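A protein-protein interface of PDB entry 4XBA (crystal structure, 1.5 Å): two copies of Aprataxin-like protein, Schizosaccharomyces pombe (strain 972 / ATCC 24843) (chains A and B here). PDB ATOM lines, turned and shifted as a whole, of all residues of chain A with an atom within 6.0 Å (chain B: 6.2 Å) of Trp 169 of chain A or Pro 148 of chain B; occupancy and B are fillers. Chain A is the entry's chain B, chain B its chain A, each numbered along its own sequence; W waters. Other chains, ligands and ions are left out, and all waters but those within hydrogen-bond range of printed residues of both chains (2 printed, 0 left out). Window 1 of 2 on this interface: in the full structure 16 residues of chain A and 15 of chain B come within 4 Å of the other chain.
Of the 16 printed residues of chain A, 5 touch a printed residue of chain B.
No position is printed for both chains.
Of the 9 pairs that touch across the chains among the printed residues, none has its exchanged pair printed and touching as well.
Trp 169 of chain A touches one residue of chain B.
Printed residues of chain B within 4 Å of Gly 172 of chain A: Pro 148 and Ser 150.
Pro 148 of chain B touches just these residues of chain A: Trp 169, Arg 170, Cys 171 and Gly 172.
Of the printed residues of chain A, Thr 149 of chain B touches Cys 171 (3.8 Å).
The nearest residue of chain A that does not touch Pro 148 of chain B is Cys 168 of chain A (5.4 Å).
The nearest printed residue of chain A that does not touch Thr 149 of chain B is Arg 170 of chain A (5.5 Å).
The backbone carbonyl oxygen of Lys 167 of chain A sits at hydrogen-bond distance from the side-chain hydroxyl of Tyr 134 of chain A (2.8 Å).
The backbone carbonyl oxygen of Leu 121 of chain A sits at hydrogen-bond distance from the indole nitrogen of Trp 169 of chain A (3.1 Å).
The side-chain hydroxyl (OG) of Ser 150 of chain B lies within hydrogen-bond range of the side-chain amide oxygen (OD1) of Asn 151 of chain B (2.8 Å).
The backbone NH (N) of Trp 169 of chain A sits at hydrogen-bond distance from the side-chain hydroxyl (OH) of Tyr 134 of chain A (3.1 Å).
OE1 of Glu 189 of chain A is in salt-bridge range of NH1 of Arg 170 of chain A, at 2.8 Å.
The side-chain sulfur (SG) of Cys 168 of chain A lies close to the backbone NH (N) of Arg 170 of chain A, at 3.3 Å.
The side-chain amide oxygen (OD1) of Asn 151 of chain B is in hydrogen-bond range of the side-chain amino group (NZ) of Lys 167 of chain A (2.9 Å).
Among the printed residues, merely in contact across the chains: Lys 167 of chain A with Ser 150 of chain B (3.7 Å), Trp 169 of chain A with Pro 148 of chain B (3.9 Å), Arg 170 of chain A with Pro 148 of chain B (3.7 Å), Cys 171 of chain A with Pro 148 of chain B (3.5 Å), Cys 171 of chain A with Thr 149 of chain B (3.8 Å), Cys 171 of chain A with Ser 150 of chain B (3.7 Å), Gly 172 of chain A with Pro 148 of chain B (3.9 Å) and Gly 172 of chain A with Ser 150 of chain B (3.3 Å).
Water W1 lies within hydrogen-bond range of O of Asp 146 of chain B (2.5 Å) and O of Arg 170 of chain A (2.7 Å).
Water W2 lies within hydrogen-bond range of the backbone carbonyl oxygen of Cys 171 of chain A (2.6 Å) and the backbone NH of Ser 150 of chain B (3.4 Å).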
ATOM      1  N   TYR A 100       1.458   9.292  -0.073  1.00  0.00           N
ATOM      2  CA  TYR A 100       0.402   8.260  -0.058  1.00  0.00           C
ATOM      3  C   TYR A 100      -0.929   8.882  -0.431  1.00  0.00           C
ATOM      4  O   TYR A 100      -1.965   8.353  -0.087  1.00  0.00           O
ATOM      5  CB  TYR A 100       0.310   7.625   1.332  1.00  0.00           C
ATOM      6  CG  TYR A 100      -0.288   6.217   1.421  1.00  0.00           C
ATOM      7  CD1 TYR A 100       0.365   5.117   0.894  1.00  0.00           C
ATOM      8  CD2 TYR A 100      -1.489   6.005   2.095  1.00  0.00           C
ATOM      9  CE1 TYR A 100      -0.176   3.839   1.003  1.00  0.00           C
ATOM     10  CE2 TYR A 100      -2.032   4.740   2.222  1.00  0.00           C
ATOM     11  CZ  TYR A 100      -1.380   3.672   1.667  1.00  0.00           C
ATOM     12  OH  TYR A 100      -1.912   2.413   1.831  1.00  0.00           O
ATOM     13  N   LYS A 102      -3.068  10.657  -3.751  1.00  0.00           N
ATOM     14  CA  LYS A 102      -3.122  10.946  -5.169  1.00  0.00           C
ATOM     15  C   LYS A 102      -4.268  11.909  -5.447  1.00  0.00           C
ATOM     16  O   LYS A 102      -5.271  11.965  -4.711  1.00  0.00           O
ATOM     17  CB  LYS A 102      -3.304   9.700  -6.018  1.00  0.00           C
ATOM     18  CG  LYS A 102      -4.509   8.883  -5.652  1.00  0.00           C
ATOM     19  CD  LYS A 102      -4.437   7.580  -6.479  1.00  0.00           C
ATOM     20  CE  LYS A 102      -5.513   6.635  -5.981  1.00  0.00           C
ATOM     21  NZ  LYS A 102      -5.339   5.301  -6.659  1.00  0.00           N
ATOM     22  N   LEU A 121      -3.835   6.155  -1.042  1.00  0.00           N
ATOM     23  CA  LEU A 121      -3.574   5.136  -2.044  1.00  0.00           C
ATOM     24  C   LEU A 121      -4.115   3.800  -1.710  1.00  0.00           C
ATOM     25  O   LEU A 121      -4.144   2.936  -2.605  1.00  0.00           O
ATOM     26  CB  LEU A 121      -2.056   4.958  -2.253  1.00  0.00           C
ATOM     27  CG  LEU A 121      -1.280   6.213  -2.666  1.00  0.00           C
ATOM     28  CD1 LEU A 121       0.149   5.810  -3.008  1.00  0.00           C
ATOM     29  CD2 LEU A 121      -1.916   6.919  -3.814  1.00  0.00           C
ATOM     30  N   ASP A 122      -4.512   3.589  -0.454  1.00  0.00           N
ATOM     31  CA  ASP A 122      -4.798   2.227   0.025  1.00  0.00           C
ATOM     32  C   ASP A 122      -5.905   1.443  -0.690  1.00  0.00           C
ATOM     33  O   ASP A 122      -5.760   0.233  -0.872  1.00  0.00           O
ATOM     34  CB  ASP A 122      -5.135   2.302   1.485  1.00  0.00           C
ATOM     35  CG  ASP A 122      -6.154   3.349   1.765  1.00  0.00           C
ATOM     36  OD1 ASP A 122      -5.763   4.507   1.991  1.00  0.00           O
ATOM     37  OD2 ASP A 122      -7.381   3.075   1.739  1.00  0.00           O
ATOM     38  N   HIS A 123      -7.001   2.115  -1.076  1.00  0.00           N
ATOM     39  CA  HIS A 123      -8.216   1.486  -1.593  1.00  0.00           C
ATOM     40  C   HIS A 123      -8.716   0.430  -0.633  1.00  0.00           C
ATOM     41  O   HIS A 123      -9.289  -0.572  -1.066  1.00  0.00           O
ATOM     42  CB  HIS A 123      -7.990   0.948  -3.002  1.00  0.00           C
ATOM     43  CG  HIS A 123      -7.869   2.062  -3.998  1.00  0.00           C
ATOM     44  ND1 HIS A 123      -8.892   2.965  -4.198  1.00  0.00           N
ATOM     45  CD2 HIS A 123      -6.848   2.460  -4.795  1.00  0.00           C
ATOM     46  CE1 HIS A 123      -8.497   3.885  -5.068  1.00  0.00           C
ATOM     47  NE2 HIS A 123      -7.267   3.593  -5.455  1.00  0.00           N
ATOM     48  N   TYR A 134     -12.357   0.160  -8.491  1.00  0.00           N
ATOM     49  CA  TYR A 134     -10.905   0.082  -8.323  1.00  0.00           C
ATOM     50  C   TYR A 134     -10.145   0.505  -9.538  1.00  0.00           C
ATOM     51  O   TYR A 134      -9.184   1.290  -9.443  1.00  0.00           O
ATOM     52  CB  TYR A 134     -10.537  -1.352  -7.938  1.00  0.00           C
ATOM     53  CG  TYR A 134      -9.062  -1.563  -7.731  1.00  0.00           C
ATOM     54  CD1 TYR A 134      -8.437  -1.108  -6.586  1.00  0.00           C
ATOM     55  CD2 TYR A 134      -8.325  -2.289  -8.662  1.00  0.00           C
ATOM     56  CE1 TYR A 134      -7.070  -1.316  -6.391  1.00  0.00           C
ATOM     57  CE2 TYR A 134      -6.954  -2.502  -8.486  1.00  0.00           C
ATOM     58  CZ  TYR A 134      -6.361  -2.018  -7.333  1.00  0.00           C
ATOM     59  OH  TYR A 134      -5.016  -2.231  -7.115  1.00  0.00           O
ATOM     60  N   THR A 138      -6.931   3.484 -10.525  1.00  0.00           N
ATOM     61  CA  THR A 138      -5.589   2.898 -10.548  1.00  0.00           C
ATOM     62  C   THR A 138      -5.092   2.625 -11.946  1.00  0.00           C
ATOM     63  O   THR A 138      -4.059   1.998 -12.116  1.00  0.00           O
ATOM     64  CB  THR A 138      -5.543   1.552  -9.776  1.00  0.00           C
ATOM     65  OG1 THR A 138      -6.538   0.649 -10.301  1.00  0.00           O
ATOM     66  CG2 THR A 138      -5.790   1.775  -8.317  1.00  0.00           C
ATOM     67  N   LYS A 167      -5.078  -5.860 -10.710  1.00  0.00           N
ATOM     68  CA  LYS A 167      -3.647  -5.802 -10.404  1.00  0.00           C
ATOM     69  C   LYS A 167      -3.438  -4.953  -9.148  1.00  0.00           C
ATOM     70  O   LYS A 167      -3.954  -3.858  -9.088  1.00  0.00           O
ATOM     71  CB  LYS A 167      -2.893  -5.207 -11.579  1.00  0.00           C
ATOM     72  CG  LYS A 167      -1.400  -5.157 -11.395  1.00  0.00           C
ATOM     73  CD  LYS A 167      -0.738  -4.677 -12.668  1.00  0.00           C
ATOM     74  CE  LYS A 167       0.789  -4.678 -12.525  1.00  0.00           C
ATOM     75  NZ  LYS A 167       1.461  -4.341 -13.811  1.00  0.00           N
ATOM     76  N   CYS A 168      -2.689  -5.443  -8.159  1.00  0.00           N
ATOM     77  CA  CYS A 168      -2.364  -4.634  -6.979  1.00  0.00           C
ATOM     78  C   CYS A 168      -1.538  -3.435  -7.422  1.00  0.00           C
ATOM     79  O   CYS A 168      -0.517  -3.632  -8.083  1.00  0.00           O
ATOM     80  CB  CYS A 168      -1.561  -5.437  -5.947  1.00  0.00           C
ATOM     81  SG  CYS A 168      -1.050  -4.376  -4.556  1.00  0.00           S
ATOM     82  N   TRP A 169      -1.934  -2.228  -7.029  1.00  0.00           N
ATOM     83  CA  TRP A 169      -1.259  -1.014  -7.481  1.00  0.00           C
ATOM     84  C   TRP A 169       0.136  -0.919  -6.889  1.00  0.00           C
ATOM     85  O   TRP A 169       1.021  -0.216  -7.416  1.00  0.00           O
ATOM     86  CB  TRP A 169      -2.089   0.216  -7.098  1.00  0.00           C
ATOM     87  CG  TRP A 169      -2.254   0.343  -5.613  1.00  0.00           C
ATOM     88  CD1 TRP A 169      -3.276  -0.169  -4.859  1.00  0.00           C
ATOM     89  CD2 TRP A 169      -1.349   0.968  -4.683  1.00  0.00           C
ATOM     90  NE1 TRP A 169      -3.069   0.130  -3.531  1.00  0.00           N
ATOM     91  CE2 TRP A 169      -1.890   0.815  -3.396  1.00  0.00           C
ATOM     92  CE3 TRP A 169      -0.120   1.645  -4.819  1.00  0.00           C
ATOM     93  CZ2 TRP A 169      -1.244   1.299  -2.248  1.00  0.00           C
ATOM     94  CZ3 TRP A 169       0.507   2.127  -3.675  1.00  0.00           C
ATOM     95  CH2 TRP A 169      -0.056   1.963  -2.428  1.00  0.00           C
ATOM     96  N   ARG A 170       0.342  -1.601  -5.777  1.00  0.00           N
ATOM     97  CA  ARG A 170       1.564  -1.425  -4.998  1.00  0.00           C
ATOM     98  C   ARG A 170       2.664  -2.405  -5.404  1.00  0.00           C
ATOM     99  O   ARG A 170       3.842  -2.029  -5.523  1.00  0.00           O
ATOM    100  CB  ARG A 170       1.259  -1.576  -3.512  1.00  0.00           C
ATOM    101  CG  ARG A 170       2.395  -1.139  -2.586  1.00  0.00           C
ATOM    102  CD  ARG A 170       1.884  -1.031  -1.158  1.00  0.00           C
ATOM    103  NE  ARG A 170       2.861  -0.389  -0.267  1.00  0.00           N
ATOM    104  CZ  ARG A 170       3.522  -0.998   0.709  1.00  0.00           C
ATOM    105  NH1 ARG A 170       3.340  -2.290   0.947  1.00  0.00           N
ATOM    106  NH2 ARG A 170       4.381  -0.307   1.452  1.00  0.00           N
ATOM    107  N   CYS A 171       2.300  -3.670  -5.601  1.00  0.00           N
ATOM    108  CA  CYS A 171       3.301  -4.698  -5.925  1.00  0.00           C
ATOM    109  C   CYS A 171       3.107  -5.318  -7.288  1.00  0.00           C
ATOM    110  O   CYS A 171       4.003  -6.008  -7.804  1.00  0.00           O
ATOM    111  CB  CYS A 171       3.326  -5.814  -4.883  1.00  0.00           C
ATOM    112  SG  CYS A 171       1.873  -6.986  -4.943  1.00  0.00           S
ATOM    113  N   GLY A 172       1.969  -5.074  -7.906  1.00  0.00           N
ATOM    114  CA  GLY A 172       1.749  -5.595  -9.241  1.00  0.00           C
ATOM    115  C   GLY A 172       1.256  -7.024  -9.380  1.00  0.00           C
ATOM    116  O   GLY A 172       1.072  -7.490 -10.496  1.00  0.00           O
ATOM    117  N   LEU A 182      -8.530  -9.611  -4.360  1.00  0.00           N
ATOM    118  CA  LEU A 182      -7.884  -8.289  -4.425  1.00  0.00           C
ATOM    119  C   LEU A 182      -8.168  -7.517  -3.132  1.00  0.00           C
ATOM    120  O   LEU A 182      -7.272  -6.933  -2.532  1.00  0.00           O
ATOM    121  CB  LEU A 182      -8.394  -7.463  -5.627  1.00  0.00           C
ATOM    122  CG  LEU A 182      -7.893  -6.007  -5.597  1.00  0.00           C
ATOM    123  CD1 LEU A 182      -6.407  -5.940  -5.838  1.00  0.00           C
ATOM    124  CD2 LEU A 182      -8.660  -5.180  -6.610  1.00  0.00           C
ATOM    125  N   LEU A 186      -5.392  -5.910  -0.618  1.00  0.00           N
ATOM    126  CA  LEU A 186      -5.239  -4.465  -0.357  1.00  0.00           C
ATOM    127  C   LEU A 186      -5.165  -4.207   1.127  1.00  0.00           C
ATOM    128  O   LEU A 186      -4.446  -3.330   1.582  1.00  0.00           O
ATOM    129  CB  LEU A 186      -6.396  -3.670  -0.979  1.00  0.00           C
ATOM    130  CG  LEU A 186      -6.368  -3.654  -2.515  1.00  0.00           C
ATOM    131  CD1 LEU A 186      -7.630  -3.036  -3.096  1.00  0.00           C
ATOM    132  CD2 LEU A 186      -5.122  -2.919  -3.026  1.00  0.00           C
ATOM    133  N   GLU A 189      -1.718  -5.039   2.202  1.00  0.00           N
ATOM    134  CA  GLU A 189      -0.769  -4.010   1.739  1.00  0.00           C
ATOM    135  C   GLU A 189      -0.838  -2.748   2.609  1.00  0.00           C
ATOM    136  O   GLU A 189       0.161  -2.082   2.882  1.00  0.00           O
ATOM    137  CB  GLU A 189      -1.031  -3.624   0.274  1.00  0.00           C
ATOM    138  CG  GLU A 189      -0.629  -4.688  -0.773  1.00  0.00           C
ATOM    139  CD  GLU A 189       0.890  -4.748  -1.042  1.00  0.00           C
ATOM    140  OE1 GLU A 189       1.686  -4.249  -0.217  1.00  0.00           O
ATOM    141  OE2 GLU A 189       1.278  -5.331  -2.067  1.00  0.00           O
ATOM    142  N   ARG B  62      14.966  -7.342  -1.527  1.00  0.00           N
ATOM    143  CA  ARG B  62      13.989  -6.426  -0.970  1.00  0.00           C
ATOM    144  C   ARG B  62      14.361  -5.977   0.427  1.00  0.00           C
ATOM    145  O   ARG B  62      13.889  -4.907   0.845  1.00  0.00           O
ATOM    146  CB  ARG B  62      12.594  -7.086  -0.939  1.00  0.00           C
ATOM    147  CG  ARG B  62      12.049  -7.487  -2.285  1.00  0.00           C
ATOM    148  CD  ARG B  62      12.073  -6.341  -3.301  1.00  0.00           C
ATOM    149  NE  ARG B  62      11.218  -5.237  -2.836  1.00  0.00           N
ATOM    150  CZ  ARG B  62      10.985  -4.135  -3.546  1.00  0.00           C
ATOM    151  NH1 ARG B  62      11.555  -3.994  -4.732  1.00  0.00           N
ATOM    152  NH2 ARG B  62      10.173  -3.200  -3.078  1.00  0.00           N
ATOM    153  N   LYS B 144      12.114   4.136 -10.284  1.00  0.00           N
ATOM    154  CA  LYS B 144      11.743   4.677  -8.980  1.00  0.00           C
ATOM    155  C   LYS B 144      11.773   3.598  -7.923  1.00  0.00           C
ATOM    156  O   LYS B 144      11.487   2.420  -8.205  1.00  0.00           O
ATOM    157  CB  LYS B 144      10.357   5.320  -9.029  1.00  0.00           C
ATOM    158  CG  LYS B 144      10.433   6.660  -9.795  1.00  0.00           C
ATOM    159  CD  LYS B 144       9.125   7.379  -9.925  1.00  0.00           C
ATOM    160  CE  LYS B 144       9.426   8.790 -10.445  1.00  0.00           C
ATOM    161  NZ  LYS B 144       8.228   9.640 -10.592  1.00  0.00           N
ATOM    162  N   ASP B 146       9.888   2.843  -5.543  1.00  0.00           N
ATOM    163  CA  ASP B 146       8.600   2.163  -5.250  1.00  0.00           C
ATOM    164  C   ASP B 146       8.007   1.427  -6.441  1.00  0.00           C
ATOM    165  O   ASP B 146       6.828   1.054  -6.390  1.00  0.00           O
ATOM    166  CB  ASP B 146       7.588   3.158  -4.682  1.00  0.00           C
ATOM    167  CG  ASP B 146       7.219   4.256  -5.647  1.00  0.00           C
ATOM    168  OD1 ASP B 146       7.890   4.391  -6.685  1.00  0.00           O
ATOM    169  OD2 ASP B 146       6.268   5.018  -5.349  1.00  0.00           O
ATOM    170  N   THR B 147       8.794   1.199  -7.495  1.00  0.00           N
ATOM    171  CA  THR B 147       8.299   0.449  -8.695  1.00  0.00           C
ATOM    172  C   THR B 147       7.878  -0.930  -8.297  1.00  0.00           C
ATOM    173  O   THR B 147       8.674  -1.657  -7.722  1.00  0.00           O
ATOM    174  CB  THR B 147       9.382   0.332  -9.779  1.00  0.00           C
ATOM    175  OG1 THR B 147       9.761   1.673 -10.152  1.00  0.00           O
ATOM    176  CG2 THR B 147       8.892  -0.372 -11.046  1.00  0.00           C
ATOM    177  N   PRO B 148       6.643  -1.340  -8.684  1.00  0.00           N
ATOM    178  CA  PRO B 148       6.275  -2.733  -8.453  1.00  0.00           C
ATOM    179  C   PRO B 148       7.231  -3.708  -9.116  1.00  0.00           C
ATOM    180  O   PRO B 148       7.678  -3.487 -10.241  1.00  0.00           O
ATOM    181  CB  PRO B 148       4.885  -2.829  -9.092  1.00  0.00           C
ATOM    182  CG  PRO B 148       4.346  -1.464  -9.096  1.00  0.00           C
ATOM    183  CD  PRO B 148       5.547  -0.545  -9.250  1.00  0.00           C
ATOM    184  N   THR B 149       7.529  -4.820  -8.458  1.00  0.00           N
ATOM    185  CA  THR B 149       8.490  -5.733  -9.032  1.00  0.00           C
ATOM    186  C   THR B 149       8.023  -6.324 -10.385  1.00  0.00           C
ATOM    187  O   THR B 149       8.829  -6.599 -11.285  1.00  0.00           O
ATOM    188  CB  THR B 149       8.768  -6.832  -7.998  1.00  0.00           C
ATOM    189  OG1 THR B 149       9.347  -6.233  -6.830  1.00  0.00           O
ATOM    190  CG2 THR B 149       9.719  -7.799  -8.522  1.00  0.00           C
ATOM    191  N   SER B 150       6.717  -6.409 -10.580  1.00  0.00           N
ATOM    192  CA  SER B 150       6.196  -6.865 -11.863  1.00  0.00           C
ATOM    193  C   SER B 150       6.512  -5.935 -13.027  1.00  0.00           C
ATOM    194  O   SER B 150       6.428  -6.320 -14.223  1.00  0.00           O
ATOM    195  CB  SER B 150       4.668  -7.016 -11.761  1.00  0.00           C
ATOM    196  OG  SER B 150       4.128  -5.733 -11.462  1.00  0.00           O
ATOM    197  N   ASN B 151       6.796  -4.692 -12.685  1.00  0.00           N
ATOM    198  CA  ASN B 151       6.966  -3.605 -13.652  1.00  0.00           C
ATOM    199  C   ASN B 151       8.395  -3.194 -13.878  1.00  0.00           C
ATOM    200  O   ASN B 151       8.638  -2.151 -14.480  1.00  0.00           O
ATOM    201  CB  ASN B 151       6.190  -2.354 -13.222  1.00  0.00           C
ATOM    202  CG  ASN B 151       4.691  -2.588 -13.174  1.00  0.00           C
ATOM    203  OD1 ASN B 151       4.219  -3.687 -13.427  1.00  0.00           O
ATOM    204  ND2 ASN B 151       3.946  -1.556 -12.807  1.00  0.00           N
ATOM    205  N   LEU B 152       9.362  -3.952 -13.357  1.00  0.00           N
ATOM    206  CA  LEU B 152      10.717  -3.502 -13.562  1.00  0.00           C
ATOM    207  C   LEU B 152      11.146  -3.563 -15.009  1.00  0.00           C
ATOM    208  O   LEU B 152      10.821  -4.509 -15.709  1.00  0.00           O
ATOM    209  CB  LEU B 152      11.698  -4.302 -12.730  1.00  0.00           C
ATOM    210  CG  LEU B 152      11.425  -4.167 -11.235  1.00  0.00           C
ATOM    211  CD1 LEU B 152      12.209  -5.248 -10.459  1.00  0.00           C
ATOM    212  CD2 LEU B 152      11.826  -2.776 -10.800  1.00  0.00           C
HETATM  213  O   HOH W   1       4.920   0.418  -4.962  1.00  0.00           O
HETATM  214  O   HOH W   2       4.908  -8.417  -8.436  1.00  0.00           O
